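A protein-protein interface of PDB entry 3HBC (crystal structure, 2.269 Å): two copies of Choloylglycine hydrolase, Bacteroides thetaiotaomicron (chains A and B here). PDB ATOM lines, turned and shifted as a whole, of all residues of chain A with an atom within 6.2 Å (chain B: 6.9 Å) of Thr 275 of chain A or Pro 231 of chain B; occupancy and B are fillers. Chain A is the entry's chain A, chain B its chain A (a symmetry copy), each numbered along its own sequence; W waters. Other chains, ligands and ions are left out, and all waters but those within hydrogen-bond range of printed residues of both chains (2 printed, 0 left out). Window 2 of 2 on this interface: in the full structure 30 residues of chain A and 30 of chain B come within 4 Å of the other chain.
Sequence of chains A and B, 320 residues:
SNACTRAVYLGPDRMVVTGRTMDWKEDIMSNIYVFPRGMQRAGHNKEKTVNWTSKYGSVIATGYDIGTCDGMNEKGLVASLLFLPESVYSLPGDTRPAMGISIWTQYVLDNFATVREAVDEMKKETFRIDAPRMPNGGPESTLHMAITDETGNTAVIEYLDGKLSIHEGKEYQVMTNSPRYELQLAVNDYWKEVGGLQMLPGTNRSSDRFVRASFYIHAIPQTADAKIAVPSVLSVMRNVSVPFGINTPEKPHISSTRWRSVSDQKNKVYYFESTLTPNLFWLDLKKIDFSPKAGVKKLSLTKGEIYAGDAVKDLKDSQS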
ATOM      1  N   SER A 241      29.716   9.871  -7.372  1.00  0.00           N
ATOM      2  CA  SER A 241      28.690   8.857  -7.227  1.00  0.00           C
ATOM      3  C   SER A 241      28.974   7.697  -8.153  1.00  0.00           C
ATOM      4  O   SER A 241      29.748   7.825  -9.101  1.00  0.00           O
ATOM      5  CB  SER A 241      27.308   9.439  -7.518  1.00  0.00           C
ATOM      6  OG  SER A 241      27.070  10.500  -6.619  1.00  0.00           O
ATOM      7  N   VAL A 242      28.343   6.565  -7.884  1.00  0.00           N
ATOM      8  CA  VAL A 242      28.489   5.396  -8.732  1.00  0.00           C
ATOM      9  C   VAL A 242      27.247   5.293  -9.590  1.00  0.00           C
ATOM     10  O   VAL A 242      26.159   5.161  -9.068  1.00  0.00           O
ATOM     11  CB  VAL A 242      28.602   4.124  -7.884  1.00  0.00           C
ATOM     12  CG1 VAL A 242      28.720   2.901  -8.771  1.00  0.00           C
ATOM     13  CG2 VAL A 242      29.770   4.234  -6.949  1.00  0.00           C
ATOM     14  N   PHE A 244      24.006   4.316 -11.579  1.00  0.00           N
ATOM     15  CA  PHE A 244      22.977   3.438 -11.028  1.00  0.00           C
ATOM     16  C   PHE A 244      22.985   2.028 -11.583  1.00  0.00           C
ATOM     17  O   PHE A 244      23.188   1.815 -12.773  1.00  0.00           O
ATOM     18  CB  PHE A 244      21.582   4.038 -11.205  1.00  0.00           C
ATOM     19  CG  PHE A 244      20.564   3.416 -10.313  1.00  0.00           C
ATOM     20  CD1 PHE A 244      20.391   3.878  -9.014  1.00  0.00           C
ATOM     21  CD2 PHE A 244      19.822   2.326 -10.745  1.00  0.00           C
ATOM     22  CE1 PHE A 244      19.470   3.285  -8.167  1.00  0.00           C
ATOM     23  CE2 PHE A 244      18.900   1.723  -9.903  1.00  0.00           C
ATOM     24  CZ  PHE A 244      18.719   2.206  -8.614  1.00  0.00           C
ATOM     25  N   THR A 257      25.218   4.539  -6.254  1.00  0.00           N
ATOM     26  CA  THR A 257      24.683   5.591  -5.385  1.00  0.00           C
ATOM     27  C   THR A 257      23.149   5.558  -5.340  1.00  0.00           C
ATOM     28  O   THR A 257      22.478   5.453  -6.381  1.00  0.00           O
ATOM     29  CB  THR A 257      25.204   7.007  -5.779  1.00  0.00           C
ATOM     30  OG1 THR A 257      26.629   6.961  -5.941  1.00  0.00           O
ATOM     31  CG2 THR A 257      24.847   8.058  -4.707  1.00  0.00           C
ATOM     32  N   ARG A 258      22.622   5.609  -4.117  1.00  0.00           N
ATOM     33  CA  ARG A 258      21.192   5.574  -3.862  1.00  0.00           C
ATOM     34  C   ARG A 258      20.754   6.945  -3.345  1.00  0.00           C
ATOM     35  O   ARG A 258      19.711   7.445  -3.723  1.00  0.00           O
ATOM     36  CB  ARG A 258      20.855   4.484  -2.838  1.00  0.00           C
ATOM     37  CG  ARG A 258      21.592   3.176  -3.043  1.00  0.00           C
ATOM     38  CD  ARG A 258      21.457   2.702  -4.493  1.00  0.00           C
ATOM     39  NE  ARG A 258      20.181   2.043  -4.784  1.00  0.00           N
ATOM     40  CZ  ARG A 258      20.062   0.770  -5.155  1.00  0.00           C
ATOM     41  NH1 ARG A 258      21.143   0.009  -5.284  1.00  0.00           N
ATOM     42  NH2 ARG A 258      18.864   0.259  -5.405  1.00  0.00           N
ATOM     43  N   TRP A 259      21.550   7.548  -2.471  1.00  0.00           N
ATOM     44  CA  TRP A 259      21.278   8.917  -2.060  1.00  0.00           C
ATOM     45  C   TRP A 259      22.513   9.759  -1.782  1.00  0.00           C
ATOM     46  O   TRP A 259      23.619   9.243  -1.599  1.00  0.00           O
ATOM     47  CB  TRP A 259      20.283   9.011  -0.883  1.00  0.00           C
ATOM     48  CG  TRP A 259      20.637   8.286   0.397  1.00  0.00           C
ATOM     49  CD1 TRP A 259      20.044   7.148   0.879  1.00  0.00           C
ATOM     50  CD2 TRP A 259      21.615   8.673   1.387  1.00  0.00           C
ATOM     51  NE1 TRP A 259      20.606   6.792   2.090  1.00  0.00           N
ATOM     52  CE2 TRP A 259      21.566   7.708   2.425  1.00  0.00           C
ATOM     53  CE3 TRP A 259      22.528   9.729   1.494  1.00  0.00           C
ATOM     54  CZ2 TRP A 259      22.401   7.771   3.550  1.00  0.00           C
ATOM     55  CZ3 TRP A 259      23.360   9.782   2.618  1.00  0.00           C
ATOM     56  CH2 TRP A 259      23.294   8.806   3.622  1.00  0.00           C
ATOM     57  N   ARG A 260      22.286  11.071  -1.778  1.00  0.00           N
ATOM     58  CA  ARG A 260      23.284  12.068  -1.444  1.00  0.00           C
ATOM     59  C   ARG A 260      22.725  12.960  -0.363  1.00  0.00           C
ATOM     60  O   ARG A 260      21.514  13.172  -0.276  1.00  0.00           O
ATOM     61  CB  ARG A 260      23.597  12.932  -2.660  1.00  0.00           C
ATOM     62  CG  ARG A 260      24.248  12.189  -3.783  1.00  0.00           C
ATOM     63  CD  ARG A 260      24.285  13.022  -5.048  1.00  0.00           C
ATOM     64  NE  ARG A 260      24.614  12.178  -6.190  1.00  0.00           N
ATOM     65  CZ  ARG A 260      23.749  11.801  -7.121  1.00  0.00           C
ATOM     66  NH1 ARG A 260      24.156  11.020  -8.114  1.00  0.00           N
ATOM     67  NH2 ARG A 260      22.488  12.219  -7.075  1.00  0.00           N
ATOM     68  N   GLU A 273      18.928  14.065  -1.461  1.00  0.00           N
ATOM     69  CA  GLU A 273      18.325  13.647  -2.721  1.00  0.00           C
ATOM     70  C   GLU A 273      18.486  12.165  -2.903  1.00  0.00           C
ATOM     71  O   GLU A 273      19.424  11.556  -2.378  1.00  0.00           O
ATOM     72  CB  GLU A 273      18.879  14.424  -3.925  1.00  0.00           C
ATOM     73  CG  GLU A 273      20.193  13.922  -4.536  1.00  0.00           C
ATOM     74  CD  GLU A 273      20.604  14.716  -5.787  1.00  0.00           C
ATOM     75  OE1 GLU A 273      19.725  15.396  -6.362  1.00  0.00           O
ATOM     76  OE2 GLU A 273      21.795  14.670  -6.198  1.00  0.00           O
ATOM     77  N   SER A 274      17.553  11.574  -3.635  1.00  0.00           N
ATOM     78  CA  SER A 274      17.603  10.156  -3.934  1.00  0.00           C
ATOM     79  C   SER A 274      17.884   9.980  -5.416  1.00  0.00           C
ATOM     80  O   SER A 274      17.331  10.689  -6.249  1.00  0.00           O
ATOM     81  CB  SER A 274      16.288   9.475  -3.550  1.00  0.00           C
ATOM     82  OG  SER A 274      16.008   8.371  -4.393  1.00  0.00           O
ATOM     83  N   THR A 275      18.758   9.039  -5.739  1.00  0.00           N
ATOM     84  CA  THR A 275      19.088   8.768  -7.115  1.00  0.00           C
ATOM     85  C   THR A 275      17.851   8.339  -7.879  1.00  0.00           C
ATOM     86  O   THR A 275      17.777   8.512  -9.097  1.00  0.00           O
ATOM     87  CB  THR A 275      20.186   7.709  -7.199  1.00  0.00           C
ATOM     88  OG1 THR A 275      21.427   8.323  -6.832  1.00  0.00           O
ATOM     89  CG2 THR A 275      20.294   7.169  -8.611  1.00  0.00           C
ATOM     90  N   LEU A 276      16.870   7.805  -7.156  1.00  0.00           N
ATOM     91  CA  LEU A 276      15.629   7.359  -7.785  1.00  0.00           C
ATOM     92  C   LEU A 276      14.537   8.424  -7.845  1.00  0.00           C
ATOM     93  O   LEU A 276      13.660   8.366  -8.706  1.00  0.00           O
ATOM     94  CB  LEU A 276      15.098   6.102  -7.106  1.00  0.00           C
ATOM     95  CG  LEU A 276      15.855   4.853  -7.551  1.00  0.00           C
ATOM     96  CD1 LEU A 276      15.179   3.583  -7.040  1.00  0.00           C
ATOM     97  CD2 LEU A 276      15.967   4.842  -9.067  1.00  0.00           C
ATOM     98  N   THR A 277      14.586   9.390  -6.935  1.00  0.00           N
ATOM     99  CA  THR A 277      13.554  10.422  -6.881  1.00  0.00           C
ATOM    100  C   THR A 277      14.051  11.778  -7.397  1.00  0.00           C
ATOM    101  O   THR A 277      15.147  12.234  -7.063  1.00  0.00           O
ATOM    102  CB  THR A 277      12.945  10.557  -5.469  1.00  0.00           C
ATOM    103  OG1 THR A 277      13.976  10.875  -4.527  1.00  0.00           O
ATOM    104  CG2 THR A 277      12.273   9.254  -5.053  1.00  0.00           C
ATOM    105  N   PRO A 278      13.219  12.438  -8.208  1.00  0.00           N
ATOM    106  CA  PRO A 278      13.561  13.636  -8.989  1.00  0.00           C
ATOM    107  C   PRO A 278      14.339  14.751  -8.262  1.00  0.00           C
ATOM    108  O   PRO A 278      15.310  15.248  -8.826  1.00  0.00           O
ATOM    109  CB  PRO A 278      12.182  14.144  -9.459  1.00  0.00           C
ATOM    110  CG  PRO A 278      11.177  13.431  -8.555  1.00  0.00           C
ATOM    111  CD  PRO A 278      11.799  12.087  -8.377  1.00  0.00           C
ATOM    112  N   ASP B 225      11.750  -0.503 -18.056  1.00  0.00           N
ATOM    113  CA  ASP B 225      11.003   0.311 -17.103  1.00  0.00           C
ATOM    114  C   ASP B 225      11.613   1.716 -17.021  1.00  0.00           C
ATOM    115  O   ASP B 225      12.679   1.925 -16.433  1.00  0.00           O
ATOM    116  CB  ASP B 225      10.990  -0.386 -15.730  1.00  0.00           C
ATOM    117  CG  ASP B 225      10.374   0.465 -14.618  1.00  0.00           C
ATOM    118  OD1 ASP B 225      10.358  -0.012 -13.461  1.00  0.00           O
ATOM    119  OD2 ASP B 225       9.912   1.602 -14.873  1.00  0.00           O
ATOM    120  N   ALA B 226      10.924   2.682 -17.613  1.00  0.00           N
ATOM    121  CA  ALA B 226      11.399   4.053 -17.615  1.00  0.00           C
ATOM    122  C   ALA B 226      11.698   4.549 -16.211  1.00  0.00           C
ATOM    123  O   ALA B 226      12.523   5.446 -16.023  1.00  0.00           O
ATOM    124  CB  ALA B 226      10.383   4.966 -18.295  1.00  0.00           C
ATOM    125  N   LYS B 227      11.025   3.981 -15.221  1.00  0.00           N
ATOM    126  CA  LYS B 227      11.234   4.412 -13.839  1.00  0.00           C
ATOM    127  C   LYS B 227      12.653   4.058 -13.439  1.00  0.00           C
ATOM    128  O   LYS B 227      13.184   4.589 -12.466  1.00  0.00           O
ATOM    129  CB  LYS B 227      10.228   3.749 -12.882  1.00  0.00           C
ATOM    130  CG  LYS B 227       8.772   4.168 -13.110  1.00  0.00           C
ATOM    131  CD  LYS B 227       7.789   3.411 -12.206  1.00  0.00           C
ATOM    132  CE  LYS B 227       6.335   3.852 -12.475  1.00  0.00           C
ATOM    133  NZ  LYS B 227       5.334   3.475 -11.406  1.00  0.00           N
ATOM    134  N   ILE B 228      13.266   3.155 -14.201  1.00  0.00           N
ATOM    135  CA  ILE B 228      14.644   2.746 -13.947  1.00  0.00           C
ATOM    136  C   ILE B 228      15.629   3.326 -14.974  1.00  0.00           C
ATOM    137  O   ILE B 228      16.645   3.912 -14.601  1.00  0.00           O
ATOM    138  CB  ILE B 228      14.777   1.203 -13.932  1.00  0.00           C
ATOM    139  CG1 ILE B 228      13.910   0.609 -12.821  1.00  0.00           C
ATOM    140  CG2 ILE B 228      16.227   0.799 -13.718  1.00  0.00           C
ATOM    141  CD1 ILE B 228      14.223   1.196 -11.453  1.00  0.00           C
ATOM    142  N   ALA B 229      15.317   3.153 -16.256  1.00  0.00           N
ATOM    143  CA  ALA B 229      16.186   3.604 -17.340  1.00  0.00           C
ATOM    144  C   ALA B 229      16.447   5.103 -17.280  1.00  0.00           C
ATOM    145  O   ALA B 229      17.581   5.545 -17.411  1.00  0.00           O
ATOM    146  CB  ALA B 229      15.610   3.222 -18.693  1.00  0.00           C
ATOM    147  N   VAL B 230      15.406   5.895 -17.077  1.00  0.00           N
ATOM    148  CA  VAL B 230      15.597   7.343 -17.078  1.00  0.00           C
ATOM    149  C   VAL B 230      16.564   7.814 -15.995  1.00  0.00           C
ATOM    150  O   VAL B 230      17.525   8.521 -16.299  1.00  0.00           O
ATOM    151  CB  VAL B 230      14.256   8.139 -17.021  1.00  0.00           C
ATOM    152  CG1 VAL B 230      14.491   9.598 -16.580  1.00  0.00           C
ATOM    153  CG2 VAL B 230      13.556   8.071 -18.361  1.00  0.00           C
ATOM    154  N   PRO B 231      16.316   7.437 -14.732  1.00  0.00           N
ATOM    155  CA  PRO B 231      17.237   7.862 -13.665  1.00  0.00           C
ATOM    156  C   PRO B 231      18.627   7.240 -13.842  1.00  0.00           C
ATOM    157  O   PRO B 231      19.621   7.788 -13.354  1.00  0.00           O
ATOM    158  CB  PRO B 231      16.580   7.320 -12.380  1.00  0.00           C
ATOM    159  CG  PRO B 231      15.173   6.990 -12.770  1.00  0.00           C
ATOM    160  CD  PRO B 231      15.217   6.606 -14.220  1.00  0.00           C
ATOM    161  N   SER B 232      18.688   6.102 -14.527  1.00  0.00           N
ATOM    162  CA  SER B 232      19.972   5.484 -14.811  1.00  0.00           C
ATOM    163  C   SER B 232      20.752   6.327 -15.806  1.00  0.00           C
ATOM    164  O   SER B 232      21.923   6.666 -15.577  1.00  0.00           O
ATOM    165  CB  SER B 232      19.789   4.068 -15.371  1.00  0.00           C
ATOM    166  OG  SER B 232      19.428   3.174 -14.338  1.00  0.00           O
ATOM    167  N   VAL B 233      20.109   6.657 -16.921  1.00  0.00           N
ATOM    168  CA  VAL B 233      20.776   7.458 -17.933  1.00  0.00           C
ATOM    169  C   VAL B 233      21.207   8.769 -17.305  1.00  0.00           C
ATOM    170  O   VAL B 233      22.272   9.299 -17.620  1.00  0.00           O
ATOM    171  CB  VAL B 233      19.895   7.699 -19.135  1.00  0.00           C
ATOM    172  CG1 VAL B 233      20.474   8.814 -20.018  1.00  0.00           C
ATOM    173  CG2 VAL B 233      19.760   6.410 -19.918  1.00  0.00           C
ATOM    174  N   LEU B 234      20.404   9.251 -16.365  1.00  0.00           N
ATOM    175  CA  LEU B 234      20.698  10.506 -15.693  1.00  0.00           C
ATOM    176  C   LEU B 234      21.943  10.409 -14.833  1.00  0.00           C
ATOM    177  O   LEU B 234      22.680  11.390 -14.678  1.00  0.00           O
ATOM    178  CB  LEU B 234      19.523  10.939 -14.816  1.00  0.00           C
ATOM    179  CG  LEU B 234      19.690  12.357 -14.272  1.00  0.00           C
ATOM    180  CD1 LEU B 234      19.660  13.350 -15.430  1.00  0.00           C
ATOM    181  CD2 LEU B 234      18.638  12.706 -13.225  1.00  0.00           C
ATOM    182  N   SER B 235      22.167   9.237 -14.240  1.00  0.00           N
ATOM    183  CA  SER B 235      23.306   9.089 -13.346  1.00  0.00           C
ATOM    184  C   SER B 235      24.563   8.960 -14.202  1.00  0.00           C
ATOM    185  O   SER B 235      25.632   9.383 -13.798  1.00  0.00           O
ATOM    186  CB  SER B 235      23.139   7.897 -12.393  1.00  0.00           C
ATOM    187  OG  SER B 235      23.253   6.674 -13.103  1.00  0.00           O
ATOM    188  N   VAL B 236      24.430   8.393 -15.394  1.00  0.00           N
ATOM    189  CA  VAL B 236      25.536   8.461 -16.330  1.00  0.00           C
ATOM    190  C   VAL B 236      25.843   9.920 -16.684  1.00  0.00           C
ATOM    191  O   VAL B 236      26.995  10.365 -16.562  1.00  0.00           O
ATOM    192  CB  VAL B 236      25.278   7.673 -17.591  1.00  0.00           C
ATOM    193  CG1 VAL B 236      26.429   7.888 -18.580  1.00  0.00           C
ATOM    194  CG2 VAL B 236      25.122   6.201 -17.251  1.00  0.00           C
ATOM    195  N   ARG B 238      25.348  12.458 -15.023  1.00  0.00           N
ATOM    196  CA  ARG B 238      25.914  13.142 -13.867  1.00  0.00           C
ATOM    197  C   ARG B 238      27.382  12.808 -13.682  1.00  0.00           C
ATOM    198  O   ARG B 238      28.161  13.636 -13.207  1.00  0.00           O
ATOM    199  CB  ARG B 238      25.113  12.819 -12.613  1.00  0.00           C
ATOM    200  CG  ARG B 238      23.764  13.535 -12.619  1.00  0.00           C
ATOM    201  CD  ARG B 238      22.958  13.209 -11.400  1.00  0.00           C
ATOM    202  NE  ARG B 238      21.766  14.037 -11.297  1.00  0.00           N
ATOM    203  CZ  ARG B 238      20.779  13.790 -10.445  1.00  0.00           C
ATOM    204  NH1 ARG B 238      20.858  12.739  -9.632  1.00  0.00           N
ATOM    205  NH2 ARG B 238      19.716  14.589 -10.399  1.00  0.00           N
ATOM    206  N   VAL B 262      17.238  14.518 -20.623  1.00  0.00           N
ATOM    207  CA  VAL B 262      17.141  13.098 -20.918  1.00  0.00           C
ATOM    208  C   VAL B 262      15.878  12.873 -21.698  1.00  0.00           C
ATOM    209  O   VAL B 262      14.801  13.237 -21.254  1.00  0.00           O
ATOM    210  CB  VAL B 262      17.063  12.266 -19.644  1.00  0.00           C
ATOM    211  CG1 VAL B 262      17.038  10.797 -19.994  1.00  0.00           C
ATOM    212  CG2 VAL B 262      18.217  12.609 -18.722  1.00  0.00           C
ATOM    213  N   LEU B 280      14.319  17.597 -11.019  1.00  0.00           N
ATOM    214  CA  LEU B 280      14.113  17.153 -12.373  1.00  0.00           C
ATOM    215  C   LEU B 280      12.670  17.450 -12.731  1.00  0.00           C
ATOM    216  O   LEU B 280      11.763  17.058 -12.010  1.00  0.00           O
ATOM    217  CB  LEU B 280      14.356  15.642 -12.461  1.00  0.00           C
ATOM    218  CG  LEU B 280      14.396  15.020 -13.861  1.00  0.00           C
ATOM    219  CD1 LEU B 280      15.741  15.288 -14.503  1.00  0.00           C
ATOM    220  CD2 LEU B 280      14.108  13.529 -13.871  1.00  0.00           C
HETATM  221  O   HOH W   1      22.106  10.217  -9.784  1.00  0.00           O
HETATM  222  O   HOH W   2      19.797   9.376 -11.435  1.00  0.00           O
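The backbone NH (N) of Leu 280 of chain B is in hydrogen-bond range of the backbone carbonyl oxygen (O) of Pro 278 of chain A, at 3.4 Å. The guanidinium group (NH2) of Arg 260 of chain A lies close to the guanidinium group (NH1) of Arg 238 of chain B, at 3.1 Å. N of Phe 244 of chain A is in hydrogen-bond range of OG of Ser 235 of chain B (2.9 Å).
The backbone carbonyl oxygen (O) of Thr 257 of chain A is in hydrogen-bond range of the side-chain hydroxyl (OG1) of Thr 275 of chain A (3.1 Å). NH2 of Arg 260 of chain A is in salt-bridge range of OE2 of Glu 273 of chain A (2.7 Å). OG of Ser 235 of chain B lies within hydrogen-bond range of O of Ser 232 of chain B (2.8 Å). OG of Ser 241 of chain A sits at hydrogen-bond distance from NE of Arg 260 of chain A, 3.0 Å away. The side-chain hydroxyl (OG) of Ser 232 of chain B is in hydrogen-bond range of the backbone carbonyl oxygen (O) of Ile 228 of chain B (2.9 Å). The backbone carbonyl oxygen (O) of Arg 258 of chain A lies within hydrogen-bond range of the backbone NH (N) of Thr 275 of chain A (2.7 Å).
Among the printed residues, merely in contact across the chains: Phe 244 of chain A with Ser 232 of chain B (3.7 Å) and Thr 275 of chain A with Pro 231 of chain B (3.7 Å).
Of chain B, only Pro 231 (3.7 Å) comes within 4 Å of Thr 275 of chain A. Of chain A, only Thr 275 (3.7 Å) comes within 4 Å of Pro 231 of chain B. Printed residues of chain B within 4 Å of Arg 260 of chain A: Arg 238 (3.1 Å). Of the printed residues of chain A, Arg 238 of chain B touches Arg 260. Of the printed residues of chain B, Pro 278 of chain A touches Leu 280. Of the printed residues of chain B, Phe 244 of chain A touches Ser 232 and Ser 235. Printed residues of chain A within 4 Å of Leu 280 of chain B: Pro 278 (3.4 Å). Leu 276 of chain A touches none of the printed residues of chain B. The nearest residue of chain B that does not touch Thr 275 of chain A is Ser 235 of chain B (4.8 Å). The nearest printed residue of chain A that does not touch Ser 232 of chain B is Thr 275 of chain A (6.0 Å).
Hydrophobic or aromatic side chains of chain B that line the printed part of chain A: Pro 231 and Leu 280. Of the 13 printed residues of chain A, 4 touch a printed residue of chain B. Among the printed residues, 5 pairs touch across the chains.
No position is printed for both chains. Of the 5 pairs that touch across the chains among the printed residues, none has its exchanged pair printed and touching as well.
Water W2 bridges the backbone carbonyl oxygen (O) of Pro 231 of chain B (2.5 Å) and the backbone carbonyl oxygen (O) of Thr 275 of chain A (3.2 Å). Water W1 bridges the guanidinium group (NH1) of Arg 260 of chain A (2.8 Å) and the guanidinium group (NH1) of Arg 238 of chain B (2.8 Å).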
